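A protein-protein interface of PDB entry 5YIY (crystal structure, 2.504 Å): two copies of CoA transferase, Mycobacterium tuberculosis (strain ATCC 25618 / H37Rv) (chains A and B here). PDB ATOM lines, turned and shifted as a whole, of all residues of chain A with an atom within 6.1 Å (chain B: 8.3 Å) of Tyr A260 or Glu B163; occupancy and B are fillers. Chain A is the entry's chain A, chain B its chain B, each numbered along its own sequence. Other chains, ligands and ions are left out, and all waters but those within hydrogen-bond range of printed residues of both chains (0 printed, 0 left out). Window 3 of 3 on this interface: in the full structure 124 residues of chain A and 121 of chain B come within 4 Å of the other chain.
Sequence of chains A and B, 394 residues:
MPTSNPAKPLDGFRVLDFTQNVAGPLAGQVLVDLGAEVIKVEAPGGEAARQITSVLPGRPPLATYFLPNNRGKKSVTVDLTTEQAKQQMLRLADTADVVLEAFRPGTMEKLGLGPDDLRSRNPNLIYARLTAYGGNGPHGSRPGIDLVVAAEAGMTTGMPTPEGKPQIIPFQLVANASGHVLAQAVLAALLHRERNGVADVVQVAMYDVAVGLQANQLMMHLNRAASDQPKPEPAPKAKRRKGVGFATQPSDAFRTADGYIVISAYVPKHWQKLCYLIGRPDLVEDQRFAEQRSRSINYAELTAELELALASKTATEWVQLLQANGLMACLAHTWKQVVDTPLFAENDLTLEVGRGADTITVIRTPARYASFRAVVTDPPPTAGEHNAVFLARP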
ATOM      1  N   ALA A 253      23.568  -5.028 -11.161  1.00  0.00           N
ATOM      2  CA  ALA A 253      22.185  -4.812 -10.754  1.00  0.00           C
ATOM      3  C   ALA A 253      21.295  -4.808 -11.991  1.00  0.00           C
ATOM      4  O   ALA A 253      21.581  -4.114 -12.966  1.00  0.00           O
ATOM      5  CB  ALA A 253      22.046  -3.509  -9.985  1.00  0.00           C
ATOM      6  N   PHE A 254      20.217  -5.584 -11.953  1.00  0.00           N
ATOM      7  CA  PHE A 254      19.393  -5.782 -13.139  1.00  0.00           C
ATOM      8  C   PHE A 254      17.936  -5.368 -12.947  1.00  0.00           C
ATOM      9  O   PHE A 254      17.362  -5.544 -11.873  1.00  0.00           O
ATOM     10  CB  PHE A 254      19.451  -7.247 -13.577  1.00  0.00           C
ATOM     11  CG  PHE A 254      20.813  -7.693 -14.026  1.00  0.00           C
ATOM     12  CD1 PHE A 254      21.232  -7.475 -15.328  1.00  0.00           C
ATOM     13  CD2 PHE A 254      21.673  -8.332 -13.148  1.00  0.00           C
ATOM     14  CE1 PHE A 254      22.486  -7.883 -15.746  1.00  0.00           C
ATOM     15  CE2 PHE A 254      22.928  -8.743 -13.561  1.00  0.00           C
ATOM     16  CZ  PHE A 254      23.334  -8.519 -14.862  1.00  0.00           C
ATOM     17  N   ARG A 255      17.348  -4.822 -14.009  1.00  0.00           N
ATOM     18  CA  ARG A 255      15.946  -4.416 -14.009  1.00  0.00           C
ATOM     19  C   ARG A 255      15.000  -5.607 -14.053  1.00  0.00           C
ATOM     20  O   ARG A 255      15.196  -6.544 -14.825  1.00  0.00           O
ATOM     21  CB  ARG A 255      15.653  -3.501 -15.203  1.00  0.00           C
ATOM     22  CG  ARG A 255      14.320  -2.761 -15.128  1.00  0.00           C
ATOM     23  CD  ARG A 255      14.172  -1.751 -16.262  1.00  0.00           C
ATOM     24  NE  ARG A 255      12.958  -0.943 -16.140  1.00  0.00           N
ATOM     25  CZ  ARG A 255      12.885   0.255 -15.571  1.00  0.00           C
ATOM     26  NH1 ARG A 255      11.721   0.890 -15.526  1.00  0.00           N
ATOM     27  NH2 ARG A 255      13.964   0.819 -15.047  1.00  0.00           N
ATOM     28  N   THR A 256      13.970  -5.557 -13.216  1.00  0.00           N
ATOM     29  CA  THR A 256      12.929  -6.577 -13.203  1.00  0.00           C
ATOM     30  C   THR A 256      11.575  -5.926 -13.454  1.00  0.00           C
ATOM     31  O   THR A 256      11.504  -4.754 -13.824  1.00  0.00           O
ATOM     32  CB  THR A 256      12.888  -7.342 -11.867  1.00  0.00           C
ATOM     33  OG1 THR A 256      12.381  -6.484 -10.837  1.00  0.00           O
ATOM     34  CG2 THR A 256      14.278  -7.820 -11.483  1.00  0.00           C
ATOM     35  N   ASP A 258       9.456  -5.212 -11.192  1.00  0.00           N
ATOM     36  CA  ASP A 258       9.354  -4.197 -10.151  1.00  0.00           C
ATOM     37  C   ASP A 258      10.615  -4.162  -9.292  1.00  0.00           C
ATOM     38  O   ASP A 258      10.888  -5.094  -8.536  1.00  0.00           O
ATOM     39  CB  ASP A 258       8.127  -4.446  -9.272  1.00  0.00           C
ATOM     40  CG  ASP A 258       7.868  -3.312  -8.298  1.00  0.00           C
ATOM     41  OD1 ASP A 258       8.191  -2.153  -8.634  1.00  0.00           O
ATOM     42  OD2 ASP A 258       7.345  -3.579  -7.197  1.00  0.00           O
ATOM     43  N   GLY A 259      11.378  -3.081  -9.412  1.00  0.00           N
ATOM     44  CA  GLY A 259      12.600  -2.923  -8.646  1.00  0.00           C
ATOM     45  C   GLY A 259      13.801  -3.569  -9.308  1.00  0.00           C
ATOM     46  O   GLY A 259      13.698  -4.124 -10.403  1.00  0.00           O
ATOM     47  N   TYR A 260      14.945  -3.497  -8.637  1.00  0.00           N
ATOM     48  CA  TYR A 260      16.187  -4.036  -9.176  1.00  0.00           C
ATOM     49  C   TYR A 260      16.684  -5.223  -8.361  1.00  0.00           C
ATOM     50  O   TYR A 260      16.470  -5.292  -7.152  1.00  0.00           O
ATOM     51  CB  TYR A 260      17.267  -2.952  -9.216  1.00  0.00           C
ATOM     52  CG  TYR A 260      17.171  -2.024 -10.405  1.00  0.00           C
ATOM     53  CD1 TYR A 260      16.372  -0.890 -10.362  1.00  0.00           C
ATOM     54  CD2 TYR A 260      17.885  -2.279 -11.567  1.00  0.00           C
ATOM     55  CE1 TYR A 260      16.284  -0.037 -11.444  1.00  0.00           C
ATOM     56  CE2 TYR A 260      17.803  -1.432 -12.655  1.00  0.00           C
ATOM     57  CZ  TYR A 260      17.001  -0.313 -12.589  1.00  0.00           C
ATOM     58  OH  TYR A 260      16.915   0.534 -13.669  1.00  0.00           O
ATOM     59  N   ILE A 261      17.348  -6.157  -9.034  1.00  0.00           N
ATOM     60  CA  ILE A 261      17.978  -7.278  -8.352  1.00  0.00           C
ATOM     61  C   ILE A 261      19.482  -7.279  -8.625  1.00  0.00           C
ATOM     62  O   ILE A 261      19.924  -7.023  -9.746  1.00  0.00           O
ATOM     63  CB  ILE A 261      17.356  -8.634  -8.776  1.00  0.00           C
ATOM     64  CG1 ILE A 261      17.958  -9.779  -7.956  1.00  0.00           C
ATOM     65  CG2 ILE A 261      17.541  -8.885 -10.267  1.00  0.00           C
ATOM     66  CD1 ILE A 261      17.452 -11.147  -8.352  1.00  0.00           C
ATOM     67  N   VAL A 262      20.265  -7.539  -7.584  1.00  0.00           N
ATOM     68  CA  VAL A 262      21.712  -7.615  -7.719  1.00  0.00           C
ATOM     69  C   VAL A 262      22.135  -9.074  -7.810  1.00  0.00           C
ATOM     70  O   VAL A 262      21.977  -9.828  -6.855  1.00  0.00           O
ATOM     71  CB  VAL A 262      22.431  -6.938  -6.539  1.00  0.00           C
ATOM     72  CG1 VAL A 262      23.938  -7.043  -6.703  1.00  0.00           C
ATOM     73  CG2 VAL A 262      22.001  -5.485  -6.420  1.00  0.00           C
ATOM     74  N   GLU A 307      17.585  -8.999 -18.732  1.00  0.00           N
ATOM     75  CA  GLU A 307      16.490  -8.149 -18.278  1.00  0.00           C
ATOM     76  C   GLU A 307      15.189  -8.458 -19.012  1.00  0.00           C
ATOM     77  O   GLU A 307      14.101  -8.222 -18.486  1.00  0.00           O
ATOM     78  CB  GLU A 307      16.856  -6.674 -18.449  1.00  0.00           C
ATOM     79  CG  GLU A 307      17.847  -6.171 -17.413  1.00  0.00           C
ATOM     80  CD  GLU A 307      18.173  -4.701 -17.576  1.00  0.00           C
ATOM     81  OE1 GLU A 307      17.796  -4.118 -18.615  1.00  0.00           O
ATOM     82  OE2 GLU A 307      18.805  -4.128 -16.664  1.00  0.00           O
ATOM     83  N   ALA A 315      11.506  -8.094  -8.460  1.00  0.00           N
ATOM     84  CA  ALA A 315      12.840  -8.323  -7.918  1.00  0.00           C
ATOM     85  C   ALA A 315      12.792  -9.208  -6.674  1.00  0.00           C
ATOM     86  O   ALA A 315      13.667 -10.048  -6.468  1.00  0.00           O
ATOM     87  CB  ALA A 315      13.514  -7.001  -7.602  1.00  0.00           C
ATOM     88  N   VAL A 319      14.736 -12.839  -6.211  1.00  0.00           N
ATOM     89  CA  VAL A 319      15.720 -13.009  -5.144  1.00  0.00           C
ATOM     90  C   VAL A 319      15.491 -14.302  -4.367  1.00  0.00           C
ATOM     91  O   VAL A 319      16.433 -15.051  -4.106  1.00  0.00           O
ATOM     92  CB  VAL A 319      15.701 -11.816  -4.162  1.00  0.00           C
ATOM     93  CG1 VAL A 319      16.421 -12.168  -2.867  1.00  0.00           C
ATOM     94  CG2 VAL A 319      16.331 -10.594  -4.804  1.00  0.00           C
ATOM     95  N   CYS A 330      20.436 -10.532  -4.277  1.00  0.00           N
ATOM     96  CA  CYS A 330      19.768  -9.762  -3.256  1.00  0.00           C
ATOM     97  C   CYS A 330      19.174  -8.496  -3.799  1.00  0.00           C
ATOM     98  O   CYS A 330      19.343  -8.131  -4.925  1.00  0.00           O
ATOM     99  CB  CYS A 330      20.718  -9.364  -2.139  1.00  0.00           C
ATOM    100  SG  CYS A 330      21.900  -8.143  -2.636  1.00  0.00           S
ATOM    101  N   LEU A 331      18.423  -7.845  -2.954  1.00  0.00           N
ATOM    102  CA  LEU A 331      17.893  -6.547  -3.258  1.00  0.00           C
ATOM    103  C   LEU A 331      18.886  -5.521  -2.759  1.00  0.00           C
ATOM    104  O   LEU A 331      19.670  -5.797  -1.897  1.00  0.00           O
ATOM    105  CB  LEU A 331      16.589  -6.338  -2.538  1.00  0.00           C
ATOM    106  CG  LEU A 331      15.444  -7.240  -2.923  1.00  0.00           C
ATOM    107  CD1 LEU A 331      14.245  -6.794  -2.148  1.00  0.00           C
ATOM    108  CD2 LEU A 331      15.177  -7.152  -4.400  1.00  0.00           C
ATOM    109  N   ALA A 332      18.864  -4.322  -3.308  1.00  0.00           N
ATOM    110  CA  ALA A 332      19.756  -3.300  -2.833  1.00  0.00           C
ATOM    111  C   ALA A 332      18.972  -2.544  -1.796  1.00  0.00           C
ATOM    112  O   ALA A 332      18.128  -1.772  -2.111  1.00  0.00           O
ATOM    113  CB  ALA A 332      20.161  -2.400  -3.964  1.00  0.00           C
ATOM    114  N   PRO B 160      21.976   8.592  -6.447  1.00  0.00           N
ATOM    115  CA  PRO B 160      21.075   8.577  -7.605  1.00  0.00           C
ATOM    116  C   PRO B 160      21.809   8.425  -8.935  1.00  0.00           C
ATOM    117  O   PRO B 160      22.914   8.945  -9.090  1.00  0.00           O
ATOM    118  CB  PRO B 160      20.380   9.946  -7.531  1.00  0.00           C
ATOM    119  CG  PRO B 160      20.709  10.495  -6.167  1.00  0.00           C
ATOM    120  CD  PRO B 160      22.051   9.932  -5.848  1.00  0.00           C
ATOM    121  N   THR B 161      21.199   7.711  -9.876  1.00  0.00           N
ATOM    122  CA  THR B 161      21.754   7.563 -11.217  1.00  0.00           C
ATOM    123  C   THR B 161      20.770   8.080 -12.261  1.00  0.00           C
ATOM    124  O   THR B 161      19.564   8.114 -12.012  1.00  0.00           O
ATOM    125  CB  THR B 161      22.104   6.093 -11.534  1.00  0.00           C
ATOM    126  OG1 THR B 161      20.911   5.299 -11.506  1.00  0.00           O
ATOM    127  CG2 THR B 161      23.085   5.554 -10.522  1.00  0.00           C
ATOM    128  N   PRO B 162      21.281   8.491 -13.433  1.00  0.00           N
ATOM    129  CA  PRO B 162      20.410   8.967 -14.515  1.00  0.00           C
ATOM    130  C   PRO B 162      19.430   7.903 -15.003  1.00  0.00           C
ATOM    131  O   PRO B 162      18.365   8.244 -15.517  1.00  0.00           O
ATOM    132  CB  PRO B 162      21.400   9.340 -15.625  1.00  0.00           C
ATOM    133  CG  PRO B 162      22.678   9.618 -14.919  1.00  0.00           C
ATOM    134  CD  PRO B 162      22.709   8.694 -13.743  1.00  0.00           C
ATOM    135  N   GLU B 163      19.786   6.632 -14.839  1.00  0.00           N
ATOM    136  CA  GLU B 163      18.941   5.536 -15.302  1.00  0.00           C
ATOM    137  C   GLU B 163      17.992   5.051 -14.210  1.00  0.00           C
ATOM    138  O   GLU B 163      17.079   4.268 -14.475  1.00  0.00           O
ATOM    139  CB  GLU B 163      19.800   4.385 -15.802  1.00  0.00           C
ATOM    140  N   GLY B 164      18.207   5.516 -12.984  1.00  0.00           N
ATOM    141  CA  GLY B 164      17.387   5.104 -11.859  1.00  0.00           C
ATOM    142  C   GLY B 164      17.869   3.801 -11.252  1.00  0.00           C
ATOM    143  O   GLY B 164      17.271   3.278 -10.312  1.00  0.00           O
ATOM    144  N   LYS B 165      18.963   3.281 -11.797  1.00  0.00           N
ATOM    145  CA  LYS B 165      19.558   2.039 -11.322  1.00  0.00           C
ATOM    146  C   LYS B 165      20.387   2.296 -10.062  1.00  0.00           C
ATOM    147  O   LYS B 165      20.941   3.380  -9.901  1.00  0.00           O
ATOM    148  CB  LYS B 165      20.416   1.435 -12.444  1.00  0.00           C
ATOM    149  CG  LYS B 165      21.385   0.337 -12.045  1.00  0.00           C
ATOM    150  CD  LYS B 165      22.316  -0.003 -13.195  1.00  0.00           C
ATOM    151  CE  LYS B 165      23.334  -1.055 -12.792  1.00  0.00           C
ATOM    152  NZ  LYS B 165      24.339  -1.292 -13.864  1.00  0.00           N
ATOM    153  N   PRO B 166      20.457   1.307  -9.155  1.00  0.00           N
ATOM    154  CA  PRO B 166      21.288   1.435  -7.950  1.00  0.00           C
ATOM    155  C   PRO B 166      22.768   1.642  -8.271  1.00  0.00           C
ATOM    156  O   PRO B 166      23.295   0.987  -9.169  1.00  0.00           O
ATOM    157  CB  PRO B 166      21.070   0.102  -7.230  1.00  0.00           C
ATOM    158  CG  PRO B 166      19.733  -0.357  -7.688  1.00  0.00           C
ATOM    159  CD  PRO B 166      19.604   0.106  -9.109  1.00  0.00           C
ATOM    160  N   GLN B 167      23.423   2.546  -7.548  1.00  0.00           N
ATOM    161  CA  GLN B 167      24.838   2.820  -7.777  1.00  0.00           C
ATOM    162  C   GLN B 167      25.707   1.650  -7.342  1.00  0.00           C
ATOM    163  O   GLN B 167      25.712   1.271  -6.172  1.00  0.00           O
ATOM    164  CB  GLN B 167      25.280   4.083  -7.032  1.00  0.00           C
ATOM    165  CG  GLN B 167      25.300   5.353  -7.870  1.00  0.00           C
ATOM    166  CD  GLN B 167      26.474   5.425  -8.833  1.00  0.00           C
ATOM    167  OE1 GLN B 167      27.176   4.439  -9.059  1.00  0.00           O
ATOM    168  NE2 GLN B 167      26.695   6.605  -9.401  1.00  0.00           N
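NH2 of Arg A255 lies within hydrogen-bond range of OH of Tyr A260 (3.3 Å). The side-chain hydroxyl of Thr B161 is in hydrogen-bond range of the backbone NH of Gly B164 (3.1 Å). OG1 of Thr B161 sits at hydrogen-bond distance from O of Lys B165 (2.5 Å).
Tyr A260 touches just these residues of chain B: Glu B163, Gly B164, Lys B165 and Pro B166. Of chain A, only Tyr A260 comes within 4 Å of Glu B163. No residue of chain B comes within 4 Å of Gly A259. Printed residues of chain A within 4 Å of Lys B165: Ala A253 and Tyr A260. Of the printed residues of chain A, Gly B164 touches Tyr A260 (3.6 Å). Of the printed residues of chain B, Ala A253 touches Lys B165 (3.5 Å). Thr B161 touches none of the printed residues of chain A. Glu A307 touches none of the printed residues of chain B.
Among the printed residues, pairs that only touch across the chains: Ala A253 with Lys B165, Tyr A260 with Glu B163, Tyr A260 with Gly B164, Tyr A260 with Lys B165 and Tyr A260 with Pro B166.
No position is printed for both chains. Of the 5 pairs that touch across the chains among the printed residues, none has its exchanged pair printed and touching as well.
Hydrophobic or aromatic side chains of chain A within 4 Å of the printed part of chain B: Ala A253 and Tyr A260. Along chain A the printed residues that touch a printed residue of chain B span positions 253 to 260. Of the 8 printed residues of chain B, 4 touch a printed residue of chain A. Hydrophobic or aromatic side chains of chain B that line the printed part of chain A: Pro B166. Among the printed residues, 5 pairs touch across the chains. Among the printed residues, no Asp or Glu carboxylate lies within 4 Å of a Lys or Arg side-chain nitrogen of the other chain.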
